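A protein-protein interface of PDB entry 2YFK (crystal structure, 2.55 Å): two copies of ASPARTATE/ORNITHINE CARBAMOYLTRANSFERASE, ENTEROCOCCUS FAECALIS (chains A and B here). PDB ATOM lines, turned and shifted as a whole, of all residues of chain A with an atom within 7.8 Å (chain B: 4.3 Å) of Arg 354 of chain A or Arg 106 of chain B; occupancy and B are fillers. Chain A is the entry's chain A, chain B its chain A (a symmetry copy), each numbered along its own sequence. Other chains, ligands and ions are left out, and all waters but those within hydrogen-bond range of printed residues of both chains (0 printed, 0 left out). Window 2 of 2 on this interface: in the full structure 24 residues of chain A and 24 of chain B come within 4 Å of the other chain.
Hydrophobic or aromatic side chains of chain A that line the printed part of chain B: Leu 331, Phe 350 and Tyr 358. Printed residues of chain B that touch a printed residue of chain A: Arg 106, Glu 107, Asn 110 and Glu 143. Among the printed residues, Asp or Glu carboxylates within 4 Å of a Lys or Arg side-chain nitrogen of the other chain: Arg 354 of chain A with Glu 143 of chain B (3.3 Å).
No position is printed for both chains.
The side-chain carboxylate (OE1) of Glu 143 of chain B lies within salt-bridge range of the guanidinium group (NH2) of Arg 354 of chain A. The guanidinium group (NH1) of Arg 106 of chain B sits close to the guanidinium group (NE) of Arg 354 of chain A, 3.0 Å away.
The backbone carbonyl oxygen (O) of Arg 106 of chain B lies within hydrogen-bond range of the side-chain amide nitrogen (ND2) of Asn 110 of chain B, at 2.7 Å. OE1 of Glu 143 of chain B lies within salt-bridge range of NH2 of Arg 106 of chain B, 2.9 Å away.
Among the printed residues, merely in contact across the chains: Leu 331 of chain A with Glu 107 of chain B (3.8 Å), Phe 350 of chain A with Glu 107 of chain B (3.98 Å), Tyr 358 of chain A with Glu 107 of chain B (3.4 Å) and Tyr 358 of chain A with Asn 110 of chain B (3.8 Å).
Arg 354 of chain A touches two residues of chain B. Arg 106 of chain B touches just one residue of chain A: Arg 354 (3.0 Å). Printed residues of chain A within 4 Å of Asn 110 of chain B: Tyr 358. Printed residues of chain B within 4 Å of Leu 331 of chain A: Glu 107. Printed residues of chain A within 4 Å of Glu 107 of chain B: Leu 331, Phe 350 and Tyr 358. Of the printed residues of chain B, Tyr 358 of chain A touches Glu 107 and Asn 110. Of the printed residues of chain B, Phe 350 of chain A touches Glu 107 (3.98 Å). Glu 103 of chain B touches none of the printed residues of chain A. Tyr 353 of chain A touches none of the printed residues of chain B. The nearest residue of chain A that does not touch Arg 106 of chain B is Tyr 358 of chain A (4.3 Å).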
ATOM      1  N   TYR A 327      -9.122 -14.696 -10.170  1.00  0.00           N
ATOM      2  CA  TYR A 327      -9.215 -15.981 -10.876  1.00  0.00           C
ATOM      3  C   TYR A 327      -8.377 -17.046 -10.149  1.00  0.00           C
ATOM      4  O   TYR A 327      -7.181 -16.857  -9.919  1.00  0.00           O
ATOM      5  CB  TYR A 327      -8.737 -15.829 -12.331  1.00  0.00           C
ATOM      6  CG  TYR A 327      -8.780 -17.105 -13.156  1.00  0.00           C
ATOM      7  CD1 TYR A 327      -7.683 -17.963 -13.205  1.00  0.00           C
ATOM      8  CD2 TYR A 327      -9.909 -17.447 -13.897  1.00  0.00           C
ATOM      9  CE1 TYR A 327      -7.708 -19.134 -13.954  1.00  0.00           C
ATOM     10  CE2 TYR A 327      -9.945 -18.619 -14.654  1.00  0.00           C
ATOM     11  CZ  TYR A 327      -8.837 -19.462 -14.671  1.00  0.00           C
ATOM     12  OH  TYR A 327      -8.859 -20.632 -15.406  1.00  0.00           O
ATOM     13  N   LEU A 331      -4.758 -25.910 -11.275  1.00  0.00           N
ATOM     14  CA  LEU A 331      -3.735 -26.163 -12.300  1.00  0.00           C
ATOM     15  C   LEU A 331      -3.497 -27.660 -12.514  1.00  0.00           C
ATOM     16  O   LEU A 331      -3.565 -28.442 -11.562  1.00  0.00           O
ATOM     17  CB  LEU A 331      -2.399 -25.468 -11.996  1.00  0.00           C
ATOM     18  CG  LEU A 331      -2.389 -23.943 -11.965  1.00  0.00           C
ATOM     19  CD1 LEU A 331      -1.048 -23.438 -11.465  1.00  0.00           C
ATOM     20  CD2 LEU A 331      -2.696 -23.386 -13.349  1.00  0.00           C
ATOM     21  N   ALA A 347      -6.840 -17.186 -23.057  1.00  0.00           N
ATOM     22  CA  ALA A 347      -5.399 -17.043 -22.821  1.00  0.00           C
ATOM     23  C   ALA A 347      -5.052 -15.757 -22.080  1.00  0.00           C
ATOM     24  O   ALA A 347      -4.320 -15.785 -21.085  1.00  0.00           O
ATOM     25  CB  ALA A 347      -4.629 -17.112 -24.138  1.00  0.00           C
ATOM     26  N   SER A 348      -5.583 -14.637 -22.564  1.00  0.00           N
ATOM     27  CA  SER A 348      -5.314 -13.329 -21.965  1.00  0.00           C
ATOM     28  C   SER A 348      -5.754 -13.266 -20.500  1.00  0.00           C
ATOM     29  O   SER A 348      -5.077 -12.657 -19.673  1.00  0.00           O
ATOM     30  CB  SER A 348      -5.976 -12.208 -22.784  1.00  0.00           C
ATOM     31  OG  SER A 348      -7.300 -12.544 -23.154  1.00  0.00           O
ATOM     32  N   VAL A 349      -6.874 -13.908 -20.178  1.00  0.00           N
ATOM     33  CA  VAL A 349      -7.337 -13.977 -18.795  1.00  0.00           C
ATOM     34  C   VAL A 349      -6.329 -14.749 -17.950  1.00  0.00           C
ATOM     35  O   VAL A 349      -5.862 -14.251 -16.926  1.00  0.00           O
ATOM     36  CB  VAL A 349      -8.731 -14.636 -18.686  1.00  0.00           C
ATOM     37  CG1 VAL A 349      -9.109 -14.863 -17.222  1.00  0.00           C
ATOM     38  CG2 VAL A 349      -9.775 -13.780 -19.385  1.00  0.00           C
ATOM     39  N   PHE A 350      -5.976 -15.953 -18.393  1.00  0.00           N
ATOM     40  CA  PHE A 350      -4.997 -16.768 -17.683  1.00  0.00           C
ATOM     41  C   PHE A 350      -3.715 -15.981 -17.451  1.00  0.00           C
ATOM     42  O   PHE A 350      -3.264 -15.857 -16.316  1.00  0.00           O
ATOM     43  CB  PHE A 350      -4.687 -18.057 -18.452  1.00  0.00           C
ATOM     44  CG  PHE A 350      -3.788 -19.012 -17.706  1.00  0.00           C
ATOM     45  CD1 PHE A 350      -2.407 -18.900 -17.791  1.00  0.00           C
ATOM     46  CD2 PHE A 350      -4.326 -20.028 -16.925  1.00  0.00           C
ATOM     47  CE1 PHE A 350      -1.573 -19.782 -17.104  1.00  0.00           C
ATOM     48  CE2 PHE A 350      -3.498 -20.918 -16.236  1.00  0.00           C
ATOM     49  CZ  PHE A 350      -2.122 -20.792 -16.329  1.00  0.00           C
ATOM     50  N   ASP A 351      -3.149 -15.429 -18.521  1.00  0.00           N
ATOM     51  CA  ASP A 351      -1.847 -14.758 -18.438  1.00  0.00           C
ATOM     52  C   ASP A 351      -1.826 -13.658 -17.384  1.00  0.00           C
ATOM     53  O   ASP A 351      -0.871 -13.551 -16.618  1.00  0.00           O
ATOM     54  CB  ASP A 351      -1.428 -14.189 -19.801  1.00  0.00           C
ATOM     55  CG  ASP A 351      -1.097 -15.280 -20.822  1.00  0.00           C
ATOM     56  OD1 ASP A 351      -0.612 -16.363 -20.420  1.00  0.00           O
ATOM     57  OD2 ASP A 351      -1.332 -15.056 -22.034  1.00  0.00           O
ATOM     58  N   ARG A 352      -2.891 -12.862 -17.326  1.00  0.00           N
ATOM     59  CA  ARG A 352      -2.955 -11.732 -16.395  1.00  0.00           C
ATOM     60  C   ARG A 352      -2.959 -12.155 -14.921  1.00  0.00           C
ATOM     61  O   ARG A 352      -2.558 -11.377 -14.063  1.00  0.00           O
ATOM     62  CB  ARG A 352      -4.171 -10.854 -16.702  1.00  0.00           C
ATOM     63  CG  ARG A 352      -4.396  -9.711 -15.709  1.00  0.00           C
ATOM     64  CD  ARG A 352      -5.269  -8.612 -16.298  1.00  0.00           C
ATOM     65  NE  ARG A 352      -6.408  -9.163 -17.033  1.00  0.00           N
ATOM     66  CZ  ARG A 352      -7.557  -9.540 -16.485  1.00  0.00           C
ATOM     67  NH1 ARG A 352      -7.760  -9.421 -15.170  1.00  0.00           N
ATOM     68  NH2 ARG A 352      -8.520 -10.033 -17.257  1.00  0.00           N
ATOM     69  N   TYR A 353      -3.416 -13.375 -14.634  1.00  0.00           N
ATOM     70  CA  TYR A 353      -3.434 -13.899 -13.258  1.00  0.00           C
ATOM     71  C   TYR A 353      -2.336 -14.940 -12.983  1.00  0.00           C
ATOM     72  O   TYR A 353      -2.263 -15.485 -11.889  1.00  0.00           O
ATOM     73  CB  TYR A 353      -4.811 -14.501 -12.938  1.00  0.00           C
ATOM     74  CG  TYR A 353      -5.924 -13.474 -12.794  1.00  0.00           C
ATOM     75  CD1 TYR A 353      -6.092 -12.759 -11.612  1.00  0.00           C
ATOM     76  CD2 TYR A 353      -6.817 -13.233 -13.830  1.00  0.00           C
ATOM     77  CE1 TYR A 353      -7.108 -11.826 -11.470  1.00  0.00           C
ATOM     78  CE2 TYR A 353      -7.840 -12.300 -13.696  1.00  0.00           C
ATOM     79  CZ  TYR A 353      -7.977 -11.601 -12.513  1.00  0.00           C
ATOM     80  OH  TYR A 353      -8.986 -10.677 -12.372  1.00  0.00           O
ATOM     81  N   ARG A 354      -1.473 -15.191 -13.962  1.00  0.00           N
ATOM     82  CA  ARG A 354      -0.445 -16.232 -13.856  1.00  0.00           C
ATOM     83  C   ARG A 354       0.337 -16.181 -12.542  1.00  0.00           C
ATOM     84  O   ARG A 354       0.524 -17.205 -11.882  1.00  0.00           O
ATOM     85  CB  ARG A 354       0.540 -16.137 -15.031  1.00  0.00           C
ATOM     86  CG  ARG A 354       1.323 -17.424 -15.254  1.00  0.00           C
ATOM     87  CD  ARG A 354       2.380 -17.308 -16.342  1.00  0.00           C
ATOM     88  NE  ARG A 354       3.201 -16.098 -16.228  1.00  0.00           N
ATOM     89  CZ  ARG A 354       4.057 -15.831 -15.233  1.00  0.00           C
ATOM     90  NH1 ARG A 354       4.224 -16.676 -14.219  1.00  0.00           N
ATOM     91  NH2 ARG A 354       4.753 -14.695 -15.248  1.00  0.00           N
ATOM     92  N   VAL A 355       0.798 -14.985 -12.182  1.00  0.00           N
ATOM     93  CA  VAL A 355       1.533 -14.779 -10.940  1.00  0.00           C
ATOM     94  C   VAL A 355       0.718 -15.248  -9.730  1.00  0.00           C
ATOM     95  O   VAL A 355       1.232 -15.983  -8.898  1.00  0.00           O
ATOM     96  CB  VAL A 355       1.940 -13.295 -10.759  1.00  0.00           C
ATOM     97  CG1 VAL A 355       2.550 -13.058  -9.382  1.00  0.00           C
ATOM     98  CG2 VAL A 355       2.915 -12.870 -11.851  1.00  0.00           C
ATOM     99  N   GLU A 356      -0.550 -14.838  -9.649  1.00  0.00           N
ATOM    100  CA  GLU A 356      -1.425 -15.223  -8.528  1.00  0.00           C
ATOM    101  C   GLU A 356      -1.692 -16.719  -8.501  1.00  0.00           C
ATOM    102  O   GLU A 356      -1.727 -17.326  -7.432  1.00  0.00           O
ATOM    103  CB  GLU A 356      -2.770 -14.486  -8.579  1.00  0.00           C
ATOM    104  CG  GLU A 356      -2.717 -13.032  -8.130  1.00  0.00           C
ATOM    105  CD  GLU A 356      -2.237 -12.072  -9.210  1.00  0.00           C
ATOM    106  OE1 GLU A 356      -1.975 -12.518 -10.351  1.00  0.00           O
ATOM    107  OE2 GLU A 356      -2.127 -10.860  -8.910  1.00  0.00           O
ATOM    108  N   LEU A 357      -1.898 -17.303  -9.682  1.00  0.00           N
ATOM    109  CA  LEU A 357      -2.171 -18.736  -9.807  1.00  0.00           C
ATOM    110  C   LEU A 357      -1.005 -19.591  -9.306  1.00  0.00           C
ATOM    111  O   LEU A 357      -1.222 -20.639  -8.695  1.00  0.00           O
ATOM    112  CB  LEU A 357      -2.481 -19.095 -11.264  1.00  0.00           C
ATOM    113  CG  LEU A 357      -3.780 -18.556 -11.864  1.00  0.00           C
ATOM    114  CD1 LEU A 357      -3.764 -18.756 -13.361  1.00  0.00           C
ATOM    115  CD2 LEU A 357      -4.998 -19.232 -11.250  1.00  0.00           C
ATOM    116  N   TYR A 358       0.223 -19.144  -9.567  1.00  0.00           N
ATOM    117  CA  TYR A 358       1.422 -19.871  -9.125  1.00  0.00           C
ATOM    118  C   TYR A 358       1.642 -19.695  -7.617  1.00  0.00           C
ATOM    119  O   TYR A 358       1.937 -20.659  -6.908  1.00  0.00           O
ATOM    120  CB  TYR A 358       2.653 -19.413  -9.912  1.00  0.00           C
ATOM    121  CG  TYR A 358       2.661 -19.816 -11.379  1.00  0.00           C
ATOM    122  CD1 TYR A 358       1.537 -20.363 -11.991  1.00  0.00           C
ATOM    123  CD2 TYR A 358       3.792 -19.619 -12.166  1.00  0.00           C
ATOM    124  CE1 TYR A 358       1.548 -20.720 -13.324  1.00  0.00           C
ATOM    125  CE2 TYR A 358       3.805 -19.982 -13.509  1.00  0.00           C
ATOM    126  CZ  TYR A 358       2.674 -20.528 -14.076  1.00  0.00           C
ATOM    127  OH  TYR A 358       2.655 -20.889 -15.399  1.00  0.00           O
ATOM    128  N   LYS A 359       1.483 -18.463  -7.137  1.00  0.00           N
ATOM    129  CA  LYS A 359       1.547 -18.164  -5.705  1.00  0.00           C
ATOM    130  C   LYS A 359       0.504 -18.995  -4.934  1.00  0.00           C
ATOM    131  O   LYS A 359       0.764 -19.456  -3.824  1.00  0.00           O
ATOM    132  CB  LYS A 359       1.348 -16.655  -5.477  1.00  0.00           C
ATOM    133  CG  LYS A 359       1.475 -16.160  -4.029  1.00  0.00           C
ATOM    134  CD  LYS A 359       2.897 -16.326  -3.437  1.00  0.00           C
ATOM    135  CE  LYS A 359       2.995 -15.715  -2.019  1.00  0.00           C
ATOM    136  NZ  LYS A 359       4.404 -15.645  -1.483  1.00  0.00           N
ATOM    137  N   GLU A 360      -0.664 -19.197  -5.539  1.00  0.00           N
ATOM    138  CA  GLU A 360      -1.709 -20.044  -4.961  1.00  0.00           C
ATOM    139  C   GLU A 360      -1.149 -21.446  -4.741  1.00  0.00           C
ATOM    140  O   GLU A 360      -1.282 -22.013  -3.665  1.00  0.00           O
ATOM    141  CB  GLU A 360      -2.941 -20.078  -5.892  1.00  0.00           C
ATOM    142  CG  GLU A 360      -4.094 -20.987  -5.472  1.00  0.00           C
ATOM    143  CD  GLU A 360      -5.134 -21.180  -6.579  1.00  0.00           C
ATOM    144  OE1 GLU A 360      -5.301 -20.278  -7.430  1.00  0.00           O
ATOM    145  OE2 GLU A 360      -5.788 -22.246  -6.610  1.00  0.00           O
ATOM    146  N   GLU B 103       2.476 -21.599 -22.115  1.00  0.00           N
ATOM    147  CA  GLU B 103       3.650 -21.664 -21.254  1.00  0.00           C
ATOM    148  C   GLU B 103       3.614 -22.888 -20.322  1.00  0.00           C
ATOM    149  O   GLU B 103       3.361 -22.762 -19.117  1.00  0.00           O
ATOM    150  CB  GLU B 103       3.777 -20.369 -20.433  1.00  0.00           C
ATOM    151  N   THR B 104       3.889 -24.065 -20.888  1.00  0.00           N
ATOM    152  CA  THR B 104       3.914 -25.322 -20.126  1.00  0.00           C
ATOM    153  C   THR B 104       5.249 -25.557 -19.391  1.00  0.00           C
ATOM    154  O   THR B 104       5.250 -26.020 -18.248  1.00  0.00           O
ATOM    155  CB  THR B 104       3.580 -26.537 -21.035  1.00  0.00           C
ATOM    156  OG1 THR B 104       3.086 -27.613 -20.231  1.00  0.00           O
ATOM    157  CG2 THR B 104       4.798 -27.014 -21.826  1.00  0.00           C
ATOM    158  N   VAL B 105       6.372 -25.241 -20.039  1.00  0.00           N
ATOM    159  CA  VAL B 105       7.701 -25.379 -19.421  1.00  0.00           C
ATOM    160  C   VAL B 105       7.863 -24.414 -18.244  1.00  0.00           C
ATOM    161  O   VAL B 105       8.422 -24.761 -17.204  1.00  0.00           O
ATOM    162  CB  VAL B 105       8.835 -25.115 -20.445  1.00  0.00           C
ATOM    163  CG1 VAL B 105      10.178 -24.946 -19.743  1.00  0.00           C
ATOM    164  CG2 VAL B 105       8.907 -26.241 -21.463  1.00  0.00           C
ATOM    165  N   ARG B 106       7.373 -23.195 -18.438  1.00  0.00           N
ATOM    166  CA  ARG B 106       7.356 -22.170 -17.403  1.00  0.00           C
ATOM    167  C   ARG B 106       6.578 -22.639 -16.175  1.00  0.00           C
ATOM    168  O   ARG B 106       7.022 -22.445 -15.047  1.00  0.00           O
ATOM    169  CB  ARG B 106       6.722 -20.909 -17.981  1.00  0.00           C
ATOM    170  CG  ARG B 106       6.635 -19.706 -17.060  1.00  0.00           C
ATOM    171  CD  ARG B 106       5.662 -18.702 -17.660  1.00  0.00           C
ATOM    172  NE  ARG B 106       6.197 -17.346 -17.696  1.00  0.00           N
ATOM    173  CZ  ARG B 106       5.616 -16.320 -18.322  1.00  0.00           C
ATOM    174  NH1 ARG B 106       4.459 -16.478 -18.971  1.00  0.00           N
ATOM    175  NH2 ARG B 106       6.199 -15.124 -18.296  1.00  0.00           N
ATOM    176  N   GLU B 107       5.420 -23.251 -16.406  1.00  0.00           N
ATOM    177  CA  GLU B 107       4.592 -23.756 -15.319  1.00  0.00           C
ATOM    178  C   GLU B 107       5.301 -24.892 -14.584  1.00  0.00           C
ATOM    179  O   GLU B 107       5.433 -24.863 -13.363  1.00  0.00           O
ATOM    180  CB  GLU B 107       3.229 -24.220 -15.842  1.00  0.00           C
ATOM    181  CG  GLU B 107       2.262 -24.616 -14.733  1.00  0.00           C
ATOM    182  CD  GLU B 107       0.825 -24.762 -15.196  1.00  0.00           C
ATOM    183  OE1 GLU B 107       0.346 -23.889 -15.953  1.00  0.00           O
ATOM    184  OE2 GLU B 107       0.173 -25.750 -14.788  1.00  0.00           O
ATOM    185  N   THR B 108       5.769 -25.879 -15.337  1.00  0.00           N
ATOM    186  CA  THR B 108       6.532 -26.987 -14.772  1.00  0.00           C
ATOM    187  C   THR B 108       7.748 -26.516 -13.969  1.00  0.00           C
ATOM    188  O   THR B 108       8.053 -27.085 -12.920  1.00  0.00           O
ATOM    189  CB  THR B 108       6.991 -27.959 -15.881  1.00  0.00           C
ATOM    190  OG1 THR B 108       5.846 -28.390 -16.628  1.00  0.00           O
ATOM    191  CG2 THR B 108       7.695 -29.174 -15.294  1.00  0.00           C
ATOM    192  N   ALA B 109       8.428 -25.477 -14.449  1.00  0.00           N
ATOM    193  CA  ALA B 109       9.610 -24.955 -13.760  1.00  0.00           C
ATOM    194  C   ALA B 109       9.289 -24.315 -12.403  1.00  0.00           C
ATOM    195  O   ALA B 109      10.020 -24.514 -11.437  1.00  0.00           O
ATOM    196  CB  ALA B 109      10.365 -23.974 -14.648  1.00  0.00           C
ATOM    197  N   ASN B 110       8.203 -23.558 -12.319  1.00  0.00           N
ATOM    198  CA  ASN B 110       7.789 -22.966 -11.042  1.00  0.00           C
ATOM    199  C   ASN B 110       7.192 -23.994 -10.068  1.00  0.00           C
ATOM    200  O   ASN B 110       7.466 -23.946  -8.879  1.00  0.00           O
ATOM    201  CB  ASN B 110       6.792 -21.822 -11.269  1.00  0.00           C
ATOM    202  CG  ASN B 110       7.440 -20.590 -11.887  1.00  0.00           C
ATOM    203  OD1 ASN B 110       7.863 -19.679 -11.173  1.00  0.00           O
ATOM    204  ND2 ASN B 110       7.526 -20.560 -13.214  1.00  0.00           N
ATOM    205  N   SER B 140      12.351 -18.821 -16.560  1.00  0.00           N
ATOM    206  CA  SER B 140      11.088 -18.986 -15.839  1.00  0.00           C
ATOM    207  C   SER B 140      11.317 -18.921 -14.340  1.00  0.00           C
ATOM    208  O   SER B 140      10.652 -18.171 -13.623  1.00  0.00           O
ATOM    209  CB  SER B 140      10.437 -20.324 -16.202  1.00  0.00           C
ATOM    210  OG  SER B 140      10.223 -20.431 -17.602  1.00  0.00           O
ATOM    211  N   GLU B 143      12.248 -15.388 -13.120  1.00  0.00           N
ATOM    212  CA  GLU B 143      11.090 -14.497 -13.028  1.00  0.00           C
ATOM    213  C   GLU B 143      10.236 -14.810 -11.801  1.00  0.00           C
ATOM    214  O   GLU B 143       9.760 -13.898 -11.123  1.00  0.00           O
ATOM    215  CB  GLU B 143      10.230 -14.572 -14.296  1.00  0.00           C
ATOM    216  CG  GLU B 143       9.096 -13.545 -14.311  1.00  0.00           C
ATOM    217  CD  GLU B 143       8.267 -13.557 -15.590  1.00  0.00           C
ATOM    218  OE1 GLU B 143       7.960 -14.660 -16.101  1.00  0.00           O
ATOM    219  OE2 GLU B 143       7.905 -12.456 -16.068  1.00  0.00           O
